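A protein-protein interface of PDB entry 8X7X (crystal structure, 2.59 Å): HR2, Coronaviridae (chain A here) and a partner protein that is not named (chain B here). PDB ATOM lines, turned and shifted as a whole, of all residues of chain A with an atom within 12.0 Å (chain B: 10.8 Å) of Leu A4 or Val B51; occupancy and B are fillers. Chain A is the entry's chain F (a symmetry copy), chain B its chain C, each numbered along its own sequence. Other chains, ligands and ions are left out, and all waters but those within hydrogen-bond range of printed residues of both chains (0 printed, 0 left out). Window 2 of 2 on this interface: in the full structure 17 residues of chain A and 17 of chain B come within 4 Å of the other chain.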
ATOM      1  N   GLY A   1      -2.882  39.438  -3.347  1.00  0.00           N
ATOM      2  CA  GLY A   1      -3.153  38.124  -3.910  1.00  0.00           C
ATOM      3  C   GLY A   1      -4.513  37.975  -4.565  1.00  0.00           C
ATOM      4  O   GLY A   1      -5.242  38.956  -4.750  1.00  0.00           O
ATOM      5  N   LYS A   2      -4.857  36.728  -4.893  1.00  0.00           N
ATOM      6  CA  LYS A   2      -5.989  36.371  -5.734  1.00  0.00           C
ATOM      7  C   LYS A   2      -7.062  35.629  -4.942  1.00  0.00           C
ATOM      8  O   LYS A   2      -6.805  35.065  -3.872  1.00  0.00           O
ATOM      9  CB  LYS A   2      -5.528  35.500  -6.909  1.00  0.00           C
ATOM     10  CG  LYS A   2      -4.721  36.245  -7.952  1.00  0.00           C
ATOM     11  CD  LYS A   2      -5.602  36.733  -9.094  1.00  0.00           C
ATOM     12  CE  LYS A   2      -5.959  35.584 -10.031  1.00  0.00           C
ATOM     13  NZ  LYS A   2      -6.834  36.024 -11.165  1.00  0.00           N
ATOM     14  N   ASN A   3      -8.277  35.619  -5.509  1.00  0.00           N
ATOM     15  CA  ASN A   3      -9.460  35.010  -4.892  1.00  0.00           C
ATOM     16  C   ASN A   3      -9.660  33.622  -5.504  1.00  0.00           C
ATOM     17  O   ASN A   3     -10.418  33.440  -6.462  1.00  0.00           O
ATOM     18  CB  ASN A   3     -10.682  35.902  -5.093  1.00  0.00           C
ATOM     19  CG  ASN A   3     -11.765  35.672  -4.043  1.00  0.00           C
ATOM     20  OD1 ASN A   3     -11.681  36.199  -2.925  1.00  0.00           O
ATOM     21  ND2 ASN A   3     -12.800  34.903  -4.404  1.00  0.00           N
ATOM     22  N   LEU A   4      -8.975  32.632  -4.932  1.00  0.00           N
ATOM     23  CA  LEU A   4      -9.029  31.268  -5.438  1.00  0.00           C
ATOM     24  C   LEU A   4     -10.460  30.755  -5.448  1.00  0.00           C
ATOM     25  O   LEU A   4     -11.150  30.782  -4.422  1.00  0.00           O
ATOM     26  CB  LEU A   4      -8.156  30.370  -4.578  1.00  0.00           C
ATOM     27  CG  LEU A   4      -6.797  30.987  -4.303  1.00  0.00           C
ATOM     28  CD1 LEU A   4      -6.084  30.199  -3.224  1.00  0.00           C
ATOM     29  CD2 LEU A   4      -5.992  31.061  -5.598  1.00  0.00           C
ATOM     30  N   THR A   5     -10.911  30.313  -6.617  1.00  0.00           N
ATOM     31  CA  THR A   5     -12.190  29.638  -6.764  1.00  0.00           C
ATOM     32  C   THR A   5     -11.962  28.327  -7.507  1.00  0.00           C
ATOM     33  O   THR A   5     -11.104  28.244  -8.397  1.00  0.00           O
ATOM     34  CB  THR A   5     -13.223  30.524  -7.492  1.00  0.00           C
ATOM     35  OG1 THR A   5     -12.649  31.069  -8.687  1.00  0.00           O
ATOM     36  CG2 THR A   5     -13.661  31.666  -6.597  1.00  0.00           C
ATOM     37  N   ALA A   6     -12.710  27.297  -7.119  1.00  0.00           N
ATOM     38  CA  ALA A   6     -12.484  25.942  -7.635  1.00  0.00           C
ATOM     39  C   ALA A   6     -13.353  25.665  -8.856  1.00  0.00           C
ATOM     40  O   ALA A   6     -12.840  25.490  -9.965  1.00  0.00           O
ATOM     41  CB  ALA A   6     -12.724  24.912  -6.528  1.00  0.00           C
ATOM     42  N   ASP A   7     -14.675  25.607  -8.669  1.00  0.00           N
ATOM     43  CA  ASP A   7     -15.623  25.290  -9.746  1.00  0.00           C
ATOM     44  C   ASP A   7     -15.258  23.960 -10.425  1.00  0.00           C
ATOM     45  O   ASP A   7     -14.830  23.894 -11.576  1.00  0.00           O
ATOM     46  CB  ASP A   7     -15.699  26.439 -10.763  1.00  0.00           C
ATOM     47  CG  ASP A   7     -16.050  27.779 -10.112  1.00  0.00           C
ATOM     48  OD1 ASP A   7     -17.180  27.912  -9.582  1.00  0.00           O
ATOM     49  OD2 ASP A   7     -15.192  28.695 -10.125  1.00  0.00           O
ATOM     50  N   MET A   8     -15.430  22.891  -9.661  1.00  0.00           N
ATOM     51  CA  MET A   8     -15.099  21.556 -10.139  1.00  0.00           C
ATOM     52  C   MET A   8     -16.306  20.917 -10.839  1.00  0.00           C
ATOM     53  O   MET A   8     -17.439  20.985 -10.346  1.00  0.00           O
ATOM     54  CB  MET A   8     -14.612  20.687  -8.978  1.00  0.00           C
ATOM     55  CG  MET A   8     -13.293  21.167  -8.380  1.00  0.00           C
ATOM     56  SD  MET A   8     -11.991  21.358  -9.628  1.00  0.00           S
ATOM     57  CE  MET A   8     -11.196  19.742  -9.634  1.00  0.00           C
ATOM     58  N   SER A   9     -16.073  20.326 -12.006  1.00  0.00           N
ATOM     59  CA  SER A   9     -17.160  19.605 -12.643  1.00  0.00           C
ATOM     60  C   SER A   9     -17.358  18.263 -11.958  1.00  0.00           C
ATOM     61  O   SER A   9     -16.414  17.655 -11.436  1.00  0.00           O
ATOM     62  CB  SER A   9     -16.900  19.411 -14.133  1.00  0.00           C
ATOM     63  OG  SER A   9     -17.136  20.624 -14.828  1.00  0.00           O
ATOM     64  N   LYS A  10     -18.613  17.836 -11.921  1.00  0.00           N
ATOM     65  CA  LYS A  10     -18.998  16.538 -11.395  1.00  0.00           C
ATOM     66  C   LYS A  10     -19.566  15.662 -12.511  1.00  0.00           C
ATOM     67  O   LYS A  10     -20.272  16.141 -13.406  1.00  0.00           O
ATOM     68  CB  LYS A  10     -20.011  16.688 -10.258  1.00  0.00           C
ATOM     69  CG  LYS A  10     -19.369  16.837  -8.885  1.00  0.00           C
ATOM     70  CD  LYS A  10     -18.660  18.174  -8.721  1.00  0.00           C
ATOM     71  CE  LYS A  10     -18.120  18.356  -7.304  1.00  0.00           C
ATOM     72  NZ  LYS A  10     -19.156  18.086  -6.269  1.00  0.00           N
ATOM     73  N   ASN B  43     -12.616  12.818  -6.019  1.00  0.00           N
ATOM     74  CA  ASN B  43     -11.432  13.645  -6.226  1.00  0.00           C
ATOM     75  C   ASN B  43     -11.818  15.112  -6.446  1.00  0.00           C
ATOM     76  O   ASN B  43     -11.156  16.024  -5.934  1.00  0.00           O
ATOM     77  CB  ASN B  43     -10.610  13.093  -7.398  1.00  0.00           C
ATOM     78  CG  ASN B  43      -9.802  11.823  -7.031  1.00  0.00           C
ATOM     79  OD1 ASN B  43      -9.927  11.260  -5.935  1.00  0.00           O
ATOM     80  ND2 ASN B  43      -8.973  11.371  -7.970  1.00  0.00           N
ATOM     81  N   ALA B  44     -12.912  15.361  -7.161  1.00  0.00           N
ATOM     82  CA  ALA B  44     -13.409  16.727  -7.310  1.00  0.00           C
ATOM     83  C   ALA B  44     -13.813  17.312  -5.960  1.00  0.00           C
ATOM     84  O   ALA B  44     -13.489  18.462  -5.650  1.00  0.00           O
ATOM     85  CB  ALA B  44     -14.602  16.758  -8.274  1.00  0.00           C
ATOM     86  N   ALA B  45     -14.544  16.535  -5.153  1.00  0.00           N
ATOM     87  CA  ALA B  45     -14.994  17.029  -3.855  1.00  0.00           C
ATOM     88  C   ALA B  45     -13.806  17.408  -2.981  1.00  0.00           C
ATOM     89  O   ALA B  45     -13.815  18.460  -2.328  1.00  0.00           O
ATOM     90  CB  ALA B  45     -15.860  15.977  -3.157  1.00  0.00           C
ATOM     91  N   GLN B  46     -12.767  16.566  -2.969  1.00  0.00           N
ATOM     92  CA  GLN B  46     -11.563  16.876  -2.203  1.00  0.00           C
ATOM     93  C   GLN B  46     -10.960  18.210  -2.635  1.00  0.00           C
ATOM     94  O   GLN B  46     -10.702  19.073  -1.793  1.00  0.00           O
ATOM     95  CB  GLN B  46     -10.536  15.745  -2.327  1.00  0.00           C
ATOM     96  CG  GLN B  46     -10.898  14.465  -1.539  1.00  0.00           C
ATOM     97  CD  GLN B  46     -11.002  14.720  -0.041  1.00  0.00           C
ATOM     98  OE1 GLN B  46     -10.341  15.613   0.478  1.00  0.00           O
ATOM     99  NE2 GLN B  46     -11.848  13.958   0.654  1.00  0.00           N
ATOM    100  N   VAL B  47     -10.750  18.410  -3.944  1.00  0.00           N
ATOM    101  CA  VAL B  47     -10.175  19.674  -4.409  1.00  0.00           C
ATOM    102  C   VAL B  47     -11.018  20.851  -3.931  1.00  0.00           C
ATOM    103  O   VAL B  47     -10.488  21.860  -3.455  1.00  0.00           O
ATOM    104  CB  VAL B  47     -10.015  19.699  -5.944  1.00  0.00           C
ATOM    105  CG1 VAL B  47      -9.590  21.109  -6.400  1.00  0.00           C
ATOM    106  CG2 VAL B  47      -8.965  18.701  -6.408  1.00  0.00           C
ATOM    107  N   GLU B  48     -12.343  20.738  -4.036  1.00  0.00           N
ATOM    108  CA  GLU B  48     -13.203  21.798  -3.533  1.00  0.00           C
ATOM    109  C   GLU B  48     -12.972  22.021  -2.039  1.00  0.00           C
ATOM    110  O   GLU B  48     -12.722  23.148  -1.598  1.00  0.00           O
ATOM    111  CB  GLU B  48     -14.663  21.475  -3.819  1.00  0.00           C
ATOM    112  CG  GLU B  48     -15.017  21.577  -5.290  1.00  0.00           C
ATOM    113  CD  GLU B  48     -16.490  21.341  -5.566  1.00  0.00           C
ATOM    114  OE1 GLU B  48     -17.003  21.940  -6.537  1.00  0.00           O
ATOM    115  OE2 GLU B  48     -17.131  20.565  -4.817  1.00  0.00           O
ATOM    116  N   SER B  49     -13.035  20.948  -1.254  1.00  0.00           N
ATOM    117  CA  SER B  49     -12.761  21.049   0.171  1.00  0.00           C
ATOM    118  C   SER B  49     -11.383  21.656   0.423  1.00  0.00           C
ATOM    119  O   SER B  49     -11.230  22.521   1.293  1.00  0.00           O
ATOM    120  CB  SER B  49     -12.889  19.661   0.810  1.00  0.00           C
ATOM    121  OG  SER B  49     -12.288  19.627   2.095  1.00  0.00           O
ATOM    122  N   LEU B  50     -10.385  21.261  -0.377  1.00  0.00           N
ATOM    123  CA  LEU B  50      -9.032  21.793  -0.230  1.00  0.00           C
ATOM    124  C   LEU B  50      -8.975  23.310  -0.457  1.00  0.00           C
ATOM    125  O   LEU B  50      -8.319  24.036   0.304  1.00  0.00           O
ATOM    126  CB  LEU B  50      -8.100  21.067  -1.193  1.00  0.00           C
ATOM    127  CG  LEU B  50      -6.766  21.740  -1.479  1.00  0.00           C
ATOM    128  CD1 LEU B  50      -5.836  21.621  -0.260  1.00  0.00           C
ATOM    129  CD2 LEU B  50      -6.126  21.166  -2.751  1.00  0.00           C
ATOM    130  N   VAL B  51      -9.665  23.818  -1.483  1.00  0.00           N
ATOM    131  CA  VAL B  51      -9.589  25.246  -1.783  1.00  0.00           C
ATOM    132  C   VAL B  51     -10.211  26.073  -0.660  1.00  0.00           C
ATOM    133  O   VAL B  51      -9.690  27.138  -0.285  1.00  0.00           O
ATOM    134  CB  VAL B  51     -10.237  25.534  -3.144  1.00  0.00           C
ATOM    135  CG1 VAL B  51     -10.695  27.011  -3.276  1.00  0.00           C
ATOM    136  CG2 VAL B  51      -9.261  25.166  -4.228  1.00  0.00           C
ATOM    137  N   SER B  52     -11.316  25.591  -0.089  1.00  0.00           N
ATOM    138  CA  SER B  52     -11.869  26.250   1.088  1.00  0.00           C
ATOM    139  C   SER B  52     -10.817  26.382   2.179  1.00  0.00           C
ATOM    140  O   SER B  52     -10.615  27.469   2.728  1.00  0.00           O
ATOM    141  CB  SER B  52     -13.081  25.489   1.608  1.00  0.00           C
ATOM    142  OG  SER B  52     -14.265  26.115   1.155  1.00  0.00           O
ATOM    143  N   GLY B  53     -10.116  25.289   2.485  1.00  0.00           N
ATOM    144  CA  GLY B  53      -9.080  25.341   3.501  1.00  0.00           C
ATOM    145  C   GLY B  53      -7.953  26.288   3.142  1.00  0.00           C
ATOM    146  O   GLY B  53      -7.439  27.010   4.001  1.00  0.00           O
ATOM    147  N   ILE B  54      -7.563  26.313   1.868  1.00  0.00           N
ATOM    148  CA  ILE B  54      -6.490  27.210   1.450  1.00  0.00           C
ATOM    149  C   ILE B  54      -6.933  28.659   1.570  1.00  0.00           C
ATOM    150  O   ILE B  54      -6.131  29.547   1.890  1.00  0.00           O
ATOM    151  CB  ILE B  54      -6.055  26.852   0.017  1.00  0.00           C
ATOM    152  CG1 ILE B  54      -5.430  25.443  -0.015  1.00  0.00           C
ATOM    153  CG2 ILE B  54      -5.081  27.872  -0.516  1.00  0.00           C
ATOM    154  CD1 ILE B  54      -5.047  24.960  -1.417  1.00  0.00           C
ATOM    155  N   THR B  55      -8.219  28.917   1.344  1.00  0.00           N
ATOM    156  CA  THR B  55      -8.747  30.270   1.451  1.00  0.00           C
ATOM    157  C   THR B  55      -8.792  30.736   2.905  1.00  0.00           C
ATOM    158  O   THR B  55      -8.418  31.882   3.202  1.00  0.00           O
ATOM    159  CB  THR B  55     -10.127  30.316   0.786  1.00  0.00           C
ATOM    160  OG1 THR B  55      -9.978  30.098  -0.628  1.00  0.00           O
ATOM    161  CG2 THR B  55     -10.786  31.648   0.993  1.00  0.00           C
ATOM    162  N   GLU B  56      -9.219  29.868   3.836  1.00  0.00           N
ATOM    163  CA  GLU B  56      -9.119  30.232   5.247  1.00  0.00           C
ATOM    164  C   GLU B  56      -7.689  30.605   5.620  1.00  0.00           C
ATOM    165  O   GLU B  56      -7.470  31.586   6.339  1.00  0.00           O
ATOM    166  CB  GLU B  56      -9.586  29.098   6.153  1.00  0.00           C
ATOM    167  CG  GLU B  56     -10.983  28.586   5.948  1.00  0.00           C
ATOM    168  CD  GLU B  56     -11.347  27.546   7.005  1.00  0.00           C
ATOM    169  OE1 GLU B  56     -11.302  27.896   8.207  1.00  0.00           O
ATOM    170  OE2 GLU B  56     -11.642  26.381   6.646  1.00  0.00           O
ATOM    171  N   ASN B  57      -6.699  29.826   5.158  1.00  0.00           N
ATOM    172  CA  ASN B  57      -5.313  30.126   5.515  1.00  0.00           C
ATOM    173  C   ASN B  57      -4.883  31.479   4.966  1.00  0.00           C
ATOM    174  O   ASN B  57      -4.240  32.268   5.675  1.00  0.00           O
ATOM    175  CB  ASN B  57      -4.365  29.043   5.021  1.00  0.00           C
ATOM    176  CG  ASN B  57      -4.402  27.806   5.878  1.00  0.00           C
ATOM    177  OD1 ASN B  57      -5.465  27.371   6.301  1.00  0.00           O
ATOM    178  ND2 ASN B  57      -3.241  27.221   6.125  1.00  0.00           N
ATOM    179  N   PHE B  58      -5.244  31.781   3.713  1.00  0.00           N
ATOM    180  CA  PHE B  58      -4.795  33.058   3.167  1.00  0.00           C
ATOM    181  C   PHE B  58      -5.445  34.221   3.889  1.00  0.00           C
ATOM    182  O   PHE B  58      -4.786  35.244   4.115  1.00  0.00           O
ATOM    183  CB  PHE B  58      -5.046  33.135   1.665  1.00  0.00           C
ATOM    184  CG  PHE B  58      -4.056  32.349   0.853  1.00  0.00           C
ATOM    185  CD1 PHE B  58      -2.716  32.375   1.177  1.00  0.00           C
ATOM    186  CD2 PHE B  58      -4.472  31.541  -0.205  1.00  0.00           C
ATOM    187  CE1 PHE B  58      -1.799  31.636   0.459  1.00  0.00           C
ATOM    188  CE2 PHE B  58      -3.549  30.817  -0.932  1.00  0.00           C
ATOM    189  CZ  PHE B  58      -2.213  30.868  -0.593  1.00  0.00           C
ATOM    190  N   GLY B  59      -6.706  34.064   4.303  1.00  0.00           N
ATOM    191  CA  GLY B  59      -7.341  35.083   5.132  1.00  0.00           C
ATOM    192  C   GLY B  59      -6.633  35.306   6.457  1.00  0.00           C
ATOM    193  O   GLY B  59      -6.346  36.444   6.827  1.00  0.00           O
ATOM    194  N   ILE B  61      -3.555  34.724   7.097  1.00  0.00           N
ATOM    195  CA  ILE B  61      -2.261  35.341   6.799  1.00  0.00           C
ATOM    196  C   ILE B  61      -2.428  36.825   6.516  1.00  0.00           C
ATOM    197  O   ILE B  61      -1.671  37.673   7.030  1.00  0.00           O
ATOM    198  CB  ILE B  61      -1.582  34.634   5.613  1.00  0.00           C
ATOM    199  CG1 ILE B  61      -1.266  33.163   5.952  1.00  0.00           C
ATOM    200  CG2 ILE B  61      -0.348  35.410   5.179  1.00  0.00           C
ATOM    201  CD1 ILE B  61      -0.952  32.298   4.738  1.00  0.00           C
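OE2 of Glu B48 lies within salt-bridge range of NZ of Lys A10 (3.5 Å).
The backbone carbonyl oxygen (O) of Val B51 is in hydrogen-bond range of the side-chain hydroxyl (OG1) of Thr B55, at 3.0 Å.
O of Leu A4 touches CG1 of Val B51 (3.97 Å).
Leu A4 touches Ile B54.
Phe B58 touches Leu A4.
Met A8 touches Ala B44 (CG to O, 3.8 Å).
CE of Met A8 touches CG1 of Val B47, 3.9 Å away.
Glu B48 touches Met A8 (CG to CG, 3.6 Å).
Ala B44 touches Ser A9.
CE of Lys A10 touches CB of Ala B44, at 3.98 Å.
Leu A4 touches just these residues of chain B: Val B51, Ile B54 and Phe B58.
Val B51 touches one residue of chain A.
No residue of chain B comes within 4 Å of Asn A3.
No residue of chain B comes within 4 Å of Thr A5.
Of chain A, only Met A8 (3.9 Å) comes within 4 Å of Val B47.
No residue of chain A comes within 4 Å of Ser B49.
No residue of chain A comes within 4 Å of Leu B50.
No residue of chain A comes within 4 Å of Ser B52.
No residue of chain A comes within 4 Å of Gly B53.
No residue of chain A comes within 4 Å of Thr B55.
Of the printed residues of chain A, Glu B48 touches Met A8 (3.6 Å) and Lys A10 (3.5 Å).
Printed residues of chain B within 4 Å of Met A8: Ala B44, Val B47 and Glu B48.
Printed residues of chain A within 4 Å of Phe B58: Leu A4 (3.5 Å).
Gly B59 touches none of the printed residues of chain A.
The nearest printed residue of chain A that does not touch Phe B58 is Lys A2 (5.6 Å).
Hydrophobic or aromatic side chains of chain A within 4 Å of the printed part of chain B: Leu A4 and Met A8.
Among the printed residues, 9 pairs touch across the chains.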
